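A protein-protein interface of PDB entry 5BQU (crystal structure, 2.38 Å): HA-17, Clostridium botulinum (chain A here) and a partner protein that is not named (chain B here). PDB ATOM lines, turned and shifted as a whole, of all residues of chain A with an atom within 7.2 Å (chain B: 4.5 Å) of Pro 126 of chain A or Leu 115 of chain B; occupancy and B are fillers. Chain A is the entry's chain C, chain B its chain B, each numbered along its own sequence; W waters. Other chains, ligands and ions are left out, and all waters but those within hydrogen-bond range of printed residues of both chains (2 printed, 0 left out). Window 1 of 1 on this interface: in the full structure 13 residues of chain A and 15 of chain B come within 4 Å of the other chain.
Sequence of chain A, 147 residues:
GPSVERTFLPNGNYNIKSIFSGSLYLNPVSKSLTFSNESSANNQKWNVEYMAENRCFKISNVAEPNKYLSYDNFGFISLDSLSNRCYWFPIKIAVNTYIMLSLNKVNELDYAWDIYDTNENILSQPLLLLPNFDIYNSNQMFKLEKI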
ATOM      1  N   SER A  32      14.156 -21.133   3.361  1.00  0.00           N
ATOM      2  CA  SER A  32      14.535 -21.081   4.759  1.00  0.00           C
ATOM      3  C   SER A  32      14.749 -22.483   5.337  1.00  0.00           C
ATOM      4  O   SER A  32      14.435 -23.480   4.707  1.00  0.00           O
ATOM      5  CB  SER A  32      13.461 -20.351   5.564  1.00  0.00           C
ATOM      6  OG  SER A  32      13.237 -19.039   5.074  1.00  0.00           O
ATOM      7  N   LEU A  33      15.321 -22.532   6.533  1.00  0.00           N
ATOM      8  CA  LEU A  33      15.512 -23.778   7.286  1.00  0.00           C
ATOM      9  C   LEU A  33      14.701 -23.674   8.560  1.00  0.00           C
ATOM     10  O   LEU A  33      14.666 -22.622   9.197  1.00  0.00           O
ATOM     11  CB  LEU A  33      16.979 -24.000   7.668  1.00  0.00           C
ATOM     12  CG  LEU A  33      17.990 -24.598   6.696  1.00  0.00           C
ATOM     13  CD1 LEU A  33      17.602 -25.990   6.273  1.00  0.00           C
ATOM     14  CD2 LEU A  33      18.232 -23.731   5.477  1.00  0.00           C
ATOM     15  N   THR A  34      14.052 -24.762   8.929  1.00  0.00           N
ATOM     16  CA  THR A  34      13.160 -24.753  10.065  1.00  0.00           C
ATOM     17  C   THR A  34      13.091 -26.153  10.619  1.00  0.00           C
ATOM     18  O   THR A  34      13.540 -27.093   9.965  1.00  0.00           O
ATOM     19  CB  THR A  34      11.762 -24.227   9.674  1.00  0.00           C
ATOM     20  OG1 THR A  34      11.118 -23.634  10.811  1.00  0.00           O
ATOM     21  CG2 THR A  34      10.882 -25.332   9.087  1.00  0.00           C
ATOM     22  N   PHE A  35      12.535 -26.279  11.821  1.00  0.00           N
ATOM     23  CA  PHE A  35      12.379 -27.560  12.491  1.00  0.00           C
ATOM     24  C   PHE A  35      10.912 -27.987  12.470  1.00  0.00           C
ATOM     25  O   PHE A  35      10.045 -27.286  12.988  1.00  0.00           O
ATOM     26  CB  PHE A  35      12.893 -27.476  13.926  1.00  0.00           C
ATOM     27  CG  PHE A  35      14.356 -27.122  14.029  1.00  0.00           C
ATOM     28  CD1 PHE A  35      15.320 -28.110  14.075  1.00  0.00           C
ATOM     29  CD2 PHE A  35      14.763 -25.796  14.093  1.00  0.00           C
ATOM     30  CE1 PHE A  35      16.665 -27.779  14.190  1.00  0.00           C
ATOM     31  CE2 PHE A  35      16.101 -25.458  14.197  1.00  0.00           C
ATOM     32  CZ  PHE A  35      17.052 -26.446  14.246  1.00  0.00           C
ATOM     33  N   PHE A  74      21.128 -11.632   4.694  1.00  0.00           N
ATOM     34  CA  PHE A  74      20.009 -11.114   5.488  1.00  0.00           C
ATOM     35  C   PHE A  74      19.897 -11.783   6.866  1.00  0.00           C
ATOM     36  O   PHE A  74      18.904 -11.590   7.579  1.00  0.00           O
ATOM     37  CB  PHE A  74      18.709 -11.255   4.672  1.00  0.00           C
ATOM     38  CG  PHE A  74      18.852 -10.768   3.272  1.00  0.00           C
ATOM     39  CD1 PHE A  74      18.694  -9.427   2.975  1.00  0.00           C
ATOM     40  CD2 PHE A  74      19.239 -11.629   2.267  1.00  0.00           C
ATOM     41  CE1 PHE A  74      18.886  -8.959   1.686  1.00  0.00           C
ATOM     42  CE2 PHE A  74      19.430 -11.171   0.968  1.00  0.00           C
ATOM     43  CZ  PHE A  74      19.260  -9.836   0.676  1.00  0.00           C
ATOM     44  N   GLY A  75      20.921 -12.555   7.241  1.00  0.00           N
ATOM     45  CA  GLY A  75      20.986 -13.209   8.556  1.00  0.00           C
ATOM     46  C   GLY A  75      20.384 -14.603   8.631  1.00  0.00           C
ATOM     47  O   GLY A  75      20.282 -15.168   9.729  1.00  0.00           O
ATOM     48  N   PHE A  76      19.971 -15.174   7.496  1.00  0.00           N
ATOM     49  CA  PHE A  76      19.351 -16.515   7.501  1.00  0.00           C
ATOM     50  C   PHE A  76      20.373 -17.561   7.150  1.00  0.00           C
ATOM     51  O   PHE A  76      21.257 -17.318   6.299  1.00  0.00           O
ATOM     52  CB  PHE A  76      18.250 -16.654   6.441  1.00  0.00           C
ATOM     53  CG  PHE A  76      17.003 -15.890   6.728  1.00  0.00           C
ATOM     54  CD1 PHE A  76      17.001 -14.519   6.742  1.00  0.00           C
ATOM     55  CD2 PHE A  76      15.807 -16.548   6.907  1.00  0.00           C
ATOM     56  CE1 PHE A  76      15.839 -13.824   6.989  1.00  0.00           C
ATOM     57  CE2 PHE A  76      14.642 -15.855   7.125  1.00  0.00           C
ATOM     58  CZ  PHE A  76      14.656 -14.493   7.179  1.00  0.00           C
ATOM     59  N   ILE A  77      20.200 -18.734   7.737  1.00  0.00           N
ATOM     60  CA  ILE A  77      20.821 -19.954   7.239  1.00  0.00           C
ATOM     61  C   ILE A  77      20.113 -20.339   5.956  1.00  0.00           C
ATOM     62  O   ILE A  77      18.918 -20.059   5.764  1.00  0.00           O
ATOM     63  CB  ILE A  77      20.722 -21.113   8.267  1.00  0.00           C
ATOM     64  CG1 ILE A  77      21.472 -20.749   9.548  1.00  0.00           C
ATOM     65  CG2 ILE A  77      21.277 -22.419   7.704  1.00  0.00           C
ATOM     66  CD1 ILE A  77      22.913 -20.377   9.305  1.00  0.00           C
ATOM     67  N   ASP A 114      21.354 -20.028  15.231  1.00  0.00           N
ATOM     68  CA  ASP A 114      20.523 -19.512  16.297  1.00  0.00           C
ATOM     69  C   ASP A 114      19.056 -19.725  15.928  1.00  0.00           C
ATOM     70  O   ASP A 114      18.609 -19.317  14.871  1.00  0.00           O
ATOM     71  CB  ASP A 114      20.831 -18.023  16.481  1.00  0.00           C
ATOM     72  CG  ASP A 114      20.360 -17.477  17.819  1.00  0.00           C
ATOM     73  OD1 ASP A 114      19.149 -17.567  18.124  1.00  0.00           O
ATOM     74  OD2 ASP A 114      21.202 -16.932  18.553  1.00  0.00           O
ATOM     75  N   ILE A 115      18.317 -20.382  16.798  1.00  0.00           N
ATOM     76  CA  ILE A 115      16.878 -20.565  16.618  1.00  0.00           C
ATOM     77  C   ILE A 115      16.155 -19.819  17.727  1.00  0.00           C
ATOM     78  O   ILE A 115      16.414 -20.043  18.917  1.00  0.00           O
ATOM     79  CB  ILE A 115      16.492 -22.055  16.583  1.00  0.00           C
ATOM     80  CG1 ILE A 115      15.047 -22.250  16.113  1.00  0.00           C
ATOM     81  CG2 ILE A 115      16.719 -22.732  17.926  1.00  0.00           C
ATOM     82  CD1 ILE A 115      14.827 -21.964  14.637  1.00  0.00           C
ATOM     83  N   TYR A 116      15.279 -18.894  17.343  1.00  0.00           N
ATOM     84  CA  TYR A 116      14.560 -18.093  18.331  1.00  0.00           C
ATOM     85  C   TYR A 116      13.431 -18.918  18.923  1.00  0.00           C
ATOM     86  O   TYR A 116      12.802 -19.716  18.214  1.00  0.00           O
ATOM     87  CB  TYR A 116      14.005 -16.819  17.715  1.00  0.00           C
ATOM     88  CG  TYR A 116      13.416 -15.835  18.692  1.00  0.00           C
ATOM     89  CD1 TYR A 116      12.032 -15.782  18.919  1.00  0.00           C
ATOM     90  CD2 TYR A 116      14.221 -14.937  19.383  1.00  0.00           C
ATOM     91  CE1 TYR A 116      11.477 -14.867  19.812  1.00  0.00           C
ATOM     92  CE2 TYR A 116      13.663 -14.021  20.288  1.00  0.00           C
ATOM     93  CZ  TYR A 116      12.294 -13.989  20.493  1.00  0.00           C
ATOM     94  OH  TYR A 116      11.729 -13.087  21.369  1.00  0.00           O
ATOM     95  N   ILE A 122       9.575 -23.289  19.240  1.00  0.00           N
ATOM     96  CA  ILE A 122      10.286 -22.882  18.013  1.00  0.00           C
ATOM     97  C   ILE A 122       9.524 -23.148  16.690  1.00  0.00           C
ATOM     98  O   ILE A 122      10.087 -23.003  15.597  1.00  0.00           O
ATOM     99  CB  ILE A 122      11.665 -23.581  17.899  1.00  0.00           C
ATOM    100  CG1 ILE A 122      11.505 -25.091  17.745  1.00  0.00           C
ATOM    101  CG2 ILE A 122      12.544 -23.264  19.090  1.00  0.00           C
ATOM    102  CD1 ILE A 122      12.804 -25.847  17.642  1.00  0.00           C
ATOM    103  N   LEU A 123       8.256 -23.532  16.772  1.00  0.00           N
ATOM    104  CA  LEU A 123       7.483 -23.835  15.569  1.00  0.00           C
ATOM    105  C   LEU A 123       7.494 -22.627  14.622  1.00  0.00           C
ATOM    106  O   LEU A 123       7.275 -21.492  15.060  1.00  0.00           O
ATOM    107  CB  LEU A 123       6.046 -24.210  15.911  1.00  0.00           C
ATOM    108  CG  LEU A 123       5.366 -25.093  14.863  1.00  0.00           C
ATOM    109  CD1 LEU A 123       6.096 -26.428  14.711  1.00  0.00           C
ATOM    110  CD2 LEU A 123       3.894 -25.318  15.198  1.00  0.00           C
ATOM    111  N   SER A 124       7.779 -22.900  13.345  1.00  0.00           N
ATOM    112  CA  SER A 124       7.774 -21.907  12.260  1.00  0.00           C
ATOM    113  C   SER A 124       8.930 -20.888  12.285  1.00  0.00           C
ATOM    114  O   SER A 124       8.921 -19.935  11.506  1.00  0.00           O
ATOM    115  CB  SER A 124       6.420 -21.174  12.197  1.00  0.00           C
ATOM    116  OG  SER A 124       5.367 -22.104  12.040  1.00  0.00           O
ATOM    117  N   GLN A 125       9.917 -21.063  13.160  1.00  0.00           N
ATOM    118  CA  GLN A 125      11.023 -20.112  13.191  1.00  0.00           C
ATOM    119  C   GLN A 125      12.048 -20.528  12.163  1.00  0.00           C
ATOM    120  O   GLN A 125      12.308 -21.710  11.997  1.00  0.00           O
ATOM    121  CB  GLN A 125      11.687 -20.072  14.567  1.00  0.00           C
ATOM    122  CG  GLN A 125      10.836 -19.455  15.668  1.00  0.00           C
ATOM    123  CD  GLN A 125      10.686 -17.950  15.565  1.00  0.00           C
ATOM    124  OE1 GLN A 125      11.278 -17.310  14.728  1.00  0.00           O
ATOM    125  NE2 GLN A 125       9.858 -17.394  16.402  1.00  0.00           N
ATOM    126  N   PRO A 126      12.643 -19.557  11.465  1.00  0.00           N
ATOM    127  CA  PRO A 126      13.780 -19.862  10.618  1.00  0.00           C
ATOM    128  C   PRO A 126      15.054 -19.912  11.428  1.00  0.00           C
ATOM    129  O   PRO A 126      15.219 -19.131  12.367  1.00  0.00           O
ATOM    130  CB  PRO A 126      13.842 -18.665   9.679  1.00  0.00           C
ATOM    131  CG  PRO A 126      13.348 -17.534  10.512  1.00  0.00           C
ATOM    132  CD  PRO A 126      12.346 -18.115  11.479  1.00  0.00           C
ATOM    133  N   LEU A 127      15.954 -20.799  11.042  1.00  0.00           N
ATOM    134  CA  LEU A 127      17.282 -20.822  11.600  1.00  0.00           C
ATOM    135  C   LEU A 127      18.088 -19.639  11.064  1.00  0.00           C
ATOM    136  O   LEU A 127      18.249 -19.464   9.833  1.00  0.00           O
ATOM    137  CB  LEU A 127      17.970 -22.138  11.251  1.00  0.00           C
ATOM    138  CG  LEU A 127      19.259 -22.466  11.991  1.00  0.00           C
ATOM    139  CD1 LEU A 127      18.972 -22.692  13.470  1.00  0.00           C
ATOM    140  CD2 LEU A 127      19.912 -23.689  11.366  1.00  0.00           C
ATOM    141  N   LEU A 128      18.594 -18.831  11.999  1.00  0.00           N
ATOM    142  CA  LEU A 128      19.386 -17.655  11.659  1.00  0.00           C
ATOM    143  C   LEU A 128      20.877 -17.792  11.993  1.00  0.00           C
ATOM    144  O   LEU A 128      21.292 -18.752  12.642  1.00  0.00           O
ATOM    145  CB  LEU A 128      18.787 -16.449  12.359  1.00  0.00           C
ATOM    146  CG  LEU A 128      17.288 -16.219  12.174  1.00  0.00           C
ATOM    147  CD1 LEU A 128      16.907 -14.953  12.900  1.00  0.00           C
ATOM    148  CD2 LEU A 128      16.891 -16.120  10.711  1.00  0.00           C
ATOM    149  N   LEU A 129      21.682 -16.839  11.510  1.00  0.00           N
ATOM    150  CA  LEU A 129      23.112 -16.766  11.860  1.00  0.00           C
ATOM    151  C   LEU A 129      23.334 -15.532  12.701  1.00  0.00           C
ATOM    152  O   LEU A 129      23.214 -14.419  12.206  1.00  0.00           O
ATOM    153  CB  LEU A 129      24.011 -16.717  10.643  1.00  0.00           C
ATOM    154  CG  LEU A 129      25.495 -16.907  10.944  1.00  0.00           C
ATOM    155  CD1 LEU A 129      25.837 -18.351  11.259  1.00  0.00           C
ATOM    156  CD2 LEU A 129      26.367 -16.444   9.790  1.00  0.00           C
ATOM    157  N   LEU A 130      23.627 -15.738  13.988  1.00  0.00           N
ATOM    158  CA  LEU A 130      23.694 -14.634  14.920  1.00  0.00           C
ATOM    159  C   LEU A 130      24.972 -14.701  15.732  1.00  0.00           C
ATOM    160  O   LEU A 130      25.681 -15.696  15.670  1.00  0.00           O
ATOM    161  CB  LEU A 130      22.456 -14.605  15.796  1.00  0.00           C
ATOM    162  CG  LEU A 130      21.164 -14.175  15.101  1.00  0.00           C
ATOM    163  CD1 LEU A 130      19.986 -14.342  16.045  1.00  0.00           C
ATOM    164  CD2 LEU A 130      21.248 -12.749  14.606  1.00  0.00           C
ATOM    165  N   TRP B  74       3.977 -11.956   8.195  1.00  0.00           N
ATOM    166  CA  TRP B  74       5.185 -12.718   7.877  1.00  0.00           C
ATOM    167  C   TRP B  74       4.866 -14.216   7.789  1.00  0.00           C
ATOM    168  O   TRP B  74       4.434 -14.846   8.758  1.00  0.00           O
ATOM    169  CB  TRP B  74       6.267 -12.459   8.918  1.00  0.00           C
ATOM    170  CG  TRP B  74       7.398 -13.407   8.829  1.00  0.00           C
ATOM    171  CD1 TRP B  74       7.906 -13.948   7.709  1.00  0.00           C
ATOM    172  CD2 TRP B  74       8.165 -13.929   9.908  1.00  0.00           C
ATOM    173  NE1 TRP B  74       8.927 -14.789   8.005  1.00  0.00           N
ATOM    174  CE2 TRP B  74       9.106 -14.807   9.356  1.00  0.00           C
ATOM    175  CE3 TRP B  74       8.148 -13.747  11.294  1.00  0.00           C
ATOM    176  CZ2 TRP B  74      10.032 -15.495  10.131  1.00  0.00           C
ATOM    177  CZ3 TRP B  74       9.069 -14.428  12.062  1.00  0.00           C
ATOM    178  CH2 TRP B  74       9.998 -15.288  11.478  1.00  0.00           C
ATOM    179  N   PRO B  77       8.189 -19.867   8.281  1.00  0.00           N
ATOM    180  CA  PRO B  77       9.569 -19.450   8.416  1.00  0.00           C
ATOM    181  C   PRO B  77      10.180 -18.833   7.164  1.00  0.00           C
ATOM    182  O   PRO B  77      11.380 -18.579   7.164  1.00  0.00           O
ATOM    183  CB  PRO B  77      10.267 -20.760   8.690  1.00  0.00           C
ATOM    184  CG  PRO B  77       9.537 -21.710   7.806  1.00  0.00           C
ATOM    185  CD  PRO B  77       8.111 -21.234   7.748  1.00  0.00           C
ATOM    186  N   ALA B 108       9.981  -4.427  13.090  1.00  0.00           N
ATOM    187  CA  ALA B 108      10.453  -5.743  13.474  1.00  0.00           C
ATOM    188  C   ALA B 108       9.297  -6.687  13.776  1.00  0.00           C
ATOM    189  O   ALA B 108       8.305  -6.277  14.336  1.00  0.00           O
ATOM    190  CB  ALA B 108      11.359  -5.624  14.691  1.00  0.00           C
ATOM    191  N   SER B 109       9.435  -7.959  13.405  1.00  0.00           N
ATOM    192  CA  SER B 109       8.400  -8.945  13.686  1.00  0.00           C
ATOM    193  C   SER B 109       8.316  -9.240  15.160  1.00  0.00           C
ATOM    194  O   SER B 109       9.313  -9.467  15.812  1.00  0.00           O
ATOM    195  CB  SER B 109       8.643 -10.271  12.948  1.00  0.00           C
ATOM    196  OG  SER B 109       7.732 -11.289  13.409  1.00  0.00           O
ATOM    197  N   ASN B 112       9.598 -12.858  15.787  1.00  0.00           N
ATOM    198  CA  ASN B 112      11.040 -12.888  15.914  1.00  0.00           C
ATOM    199  C   ASN B 112      11.574 -11.462  15.749  1.00  0.00           C
ATOM    200  O   ASN B 112      11.682 -10.971  14.634  1.00  0.00           O
ATOM    201  CB  ASN B 112      11.621 -13.829  14.864  1.00  0.00           C
ATOM    202  CG  ASN B 112      13.043 -14.242  15.167  1.00  0.00           C
ATOM    203  OD1 ASN B 112      13.826 -13.472  15.714  1.00  0.00           O
ATOM    204  ND2 ASN B 112      13.389 -15.473  14.795  1.00  0.00           N
ATOM    205  N   PRO B 113      11.868 -10.775  16.873  1.00  0.00           N
ATOM    206  CA  PRO B 113      12.330  -9.394  16.829  1.00  0.00           C
ATOM    207  C   PRO B 113      13.739  -9.214  16.289  1.00  0.00           C
ATOM    208  O   PRO B 113      14.175  -8.092  16.109  1.00  0.00           O
ATOM    209  CB  PRO B 113      12.248  -8.921  18.276  1.00  0.00           C
ATOM    210  CG  PRO B 113      11.581  -9.966  19.041  1.00  0.00           C
ATOM    211  CD  PRO B 113      11.584 -11.224  18.237  1.00  0.00           C
ATOM    212  N   ASN B 114      14.455 -10.301  16.040  1.00  0.00           N
ATOM    213  CA  ASN B 114      15.731 -10.198  15.363  1.00  0.00           C
ATOM    214  C   ASN B 114      15.499  -9.924  13.889  1.00  0.00           C
ATOM    215  O   ASN B 114      16.418  -9.524  13.211  1.00  0.00           O
ATOM    216  CB  ASN B 114      16.563 -11.468  15.515  1.00  0.00           C
ATOM    217  CG  ASN B 114      16.995 -11.719  16.939  1.00  0.00           C
ATOM    218  OD1 ASN B 114      17.872 -11.058  17.447  1.00  0.00           O
ATOM    219  ND2 ASN B 114      16.385 -12.706  17.582  1.00  0.00           N
ATOM    220  N   LEU B 115      14.274 -10.150  13.399  1.00  0.00           N
ATOM    221  CA  LEU B 115      13.974  -9.969  11.979  1.00  0.00           C
ATOM    222  C   LEU B 115      13.119  -8.759  11.737  1.00  0.00           C
ATOM    223  O   LEU B 115      12.150  -8.538  12.434  1.00  0.00           O
ATOM    224  CB  LEU B 115      13.282 -11.213  11.428  1.00  0.00           C
ATOM    225  CG  LEU B 115      14.188 -12.439  11.420  1.00  0.00           C
ATOM    226  CD1 LEU B 115      13.418 -13.662  10.956  1.00  0.00           C
ATOM    227  CD2 LEU B 115      15.403 -12.175  10.552  1.00  0.00           C
ATOM    228  N   VAL B 116      13.498  -7.974  10.735  1.00  0.00           N
ATOM    229  CA  VAL B 116      12.827  -6.733  10.423  1.00  0.00           C
ATOM    230  C   VAL B 116      12.542  -6.616   8.926  1.00  0.00           C
ATOM    231  O   VAL B 116      13.228  -7.205   8.107  1.00  0.00           O
ATOM    232  CB  VAL B 116      13.669  -5.518  10.890  1.00  0.00           C
ATOM    233  CG1 VAL B 116      14.060  -5.665  12.341  1.00  0.00           C
ATOM    234  CG2 VAL B 116      14.913  -5.336  10.036  1.00  0.00           C
ATOM    235  N   LEU B 128      12.884  -9.986   4.574  1.00  0.00           N
ATOM    236  CA  LEU B 128      13.281  -9.834   5.953  1.00  0.00           C
ATOM    237  C   LEU B 128      14.784  -9.779   6.079  1.00  0.00           C
ATOM    238  O   LEU B 128      15.499 -10.382   5.300  1.00  0.00           O
ATOM    239  CB  LEU B 128      12.719 -10.988   6.786  1.00  0.00           C
ATOM    240  CG  LEU B 128      11.227 -10.940   7.087  1.00  0.00           C
ATOM    241  CD1 LEU B 128      10.863 -12.032   8.077  1.00  0.00           C
ATOM    242  CD2 LEU B 128      10.863  -9.608   7.711  1.00  0.00           C
ATOM    243  N   SER B 129      15.249  -9.022   7.061  1.00  0.00           N
ATOM    244  CA  SER B 129      16.652  -9.014   7.420  1.00  0.00           C
ATOM    245  C   SER B 129      16.868  -8.930   8.910  1.00  0.00           C
ATOM    246  O   SER B 129      16.032  -8.429   9.638  1.00  0.00           O
ATOM    247  CB  SER B 129      17.366  -7.846   6.750  1.00  0.00           C
ATOM    248  OG  SER B 129      18.716  -7.912   7.068  1.00  0.00           O
ATOM    249  N   THR B 130      18.013  -9.422   9.365  1.00  0.00           N
ATOM    250  CA  THR B 130      18.501  -9.026  10.666  1.00  0.00           C
ATOM    251  C   THR B 130      18.881  -7.536  10.594  1.00  0.00           C
ATOM    252  O   THR B 130      19.040  -6.963   9.491  1.00  0.00           O
ATOM    253  CB  THR B 130      19.697  -9.860  11.114  1.00  0.00           C
ATOM    254  OG1 THR B 130      20.716  -9.819  10.124  1.00  0.00           O
ATOM    255  CG2 THR B 130      19.288 -11.293  11.354  1.00  0.00           C
HETATM  256  O   HOH W   1      23.020 -11.675  11.105  1.00  0.00           O
HETATM  257  O   HOH W   2      15.167 -17.863  14.865  1.00  0.00           O
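Among the printed residues, merely in contact across the chains: Tyr 116 of chain A with Asn 112 of chain B (3.3 Å), Phe 74 of chain A with Leu 128 of chain B (3.4 Å), Phe 74 of chain A with Ser 129 of chain B (3.4 Å), Pro 126 of chain A with Pro 77 of chain B (3.5 Å), Tyr 116 of chain A with Asn 114 of chain B (3.6 Å), Tyr 116 of chain A with Pro 113 of chain B (3.6 Å), Thr 34 of chain A with Pro 77 of chain B (3.7 Å), Pro 126 of chain A with Trp 74 of chain B (3.7 Å), Gly 75 of chain A with Thr 130 of chain B (3.7 Å), Phe 76 of chain A with Leu 128 of chain B (3.8 Å), Pro 126 of chain A with Leu 115 of chain B (3.9 Å), Gln 125 of chain A with Pro 77 of chain B (3.9 Å), Leu 128 of chain A with Leu 115 of chain B (3.9 Å) and Phe 76 of chain A with Leu 115 of chain B (3.95 Å).
Of the 12 printed residues of chain B, 9 touch a printed residue of chain A. Of the 20 printed residues of chain A, 10 touch a printed residue of chain B. Hydrophobic or aromatic side chains of chain A within 4 Å of the printed part of chain B: Phe 74, Phe 76, Tyr 116, Pro 126 and Leu 128.
Water W2 lies within hydrogen-bond range of N of Tyr 116 of chain A, O of Pro 126 of chain A and ND2 of Asn 112 of chain B. Water W1 bridges the backbone carbonyl oxygen of Leu 129 of chain A (3.0 Å) and the side-chain hydroxyl of Thr 130 of chain B (3.1 Å).
The backbone NH (N) of Asn 112 of chain B sits at hydrogen-bond distance from the side-chain hydroxyl (OG) of Ser 109 of chain B (3.4 Å). N of Ser 109 of chain B sits at hydrogen-bond distance from O of Leu 115 of chain B, 2.9 Å away. OD1 of Asn 112 of chain B sits close to N of Asn 114 of chain B, 3.2 Å away. The backbone NH (N) of Val 116 of chain B lies within hydrogen-bond range of the backbone carbonyl oxygen (O) of Ser 129 of chain B (2.8 Å). O of Gln 125 of chain A sits at hydrogen-bond distance from OG1 of Thr 34 of chain A. The backbone carbonyl oxygen (O) of Gly 75 of chain A sits at hydrogen-bond distance from the backbone NH (N) of Leu 129 of chain A (2.8 Å).
The side-chain hydroxyl (OG) of Ser 32 of chain A lies within hydrogen-bond range of the backbone carbonyl oxygen (O) of Pro 77 of chain B (2.8 Å). The side-chain amide nitrogen (ND2) of Asn 112 of chain B is in hydrogen-bond range of the side-chain amide oxygen (OE1) of Gln 125 of chain A (2.8 Å). The backbone NH of Thr 130 of chain B sits at hydrogen-bond distance from the backbone carbonyl oxygen of Phe 74 of chain A. The backbone nitrogen (N) of Pro 77 of chain B lies close to the backbone carbonyl oxygen (O) of Ser 124 of chain A (3.3 Å).
Pro 126 of chain A touches three residues of chain B. Leu 115 of chain B touches three residues of chain A. Of the printed residues of chain A, Pro 113 of chain B touches Tyr 116. Printed residues of chain A within 4 Å of Trp 74 of chain B: Pro 126 (3.7 Å). Of the printed residues of chain B, Tyr 116 of chain A touches Asn 112, Pro 113 and Asn 114. Printed residues of chain A within 4 Å of Leu 128 of chain B: Phe 74 (3.4 Å) and Phe 76 (3.8 Å). Ile 77 of chain A touches none of the printed residues of chain B. Leu 129 of chain A touches none of the printed residues of chain B. The nearest residue of chain B that does not touch Pro 126 of chain A is Asn 112 of chain B (4.4 Å). The nearest residue of chain A that does not touch Leu 115 of chain B is Phe 74 of chain A (4.6 Å). The nearest printed residue of chain A that does not touch Asn 114 of chain B is Leu 130 of chain A (4.1 Å).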
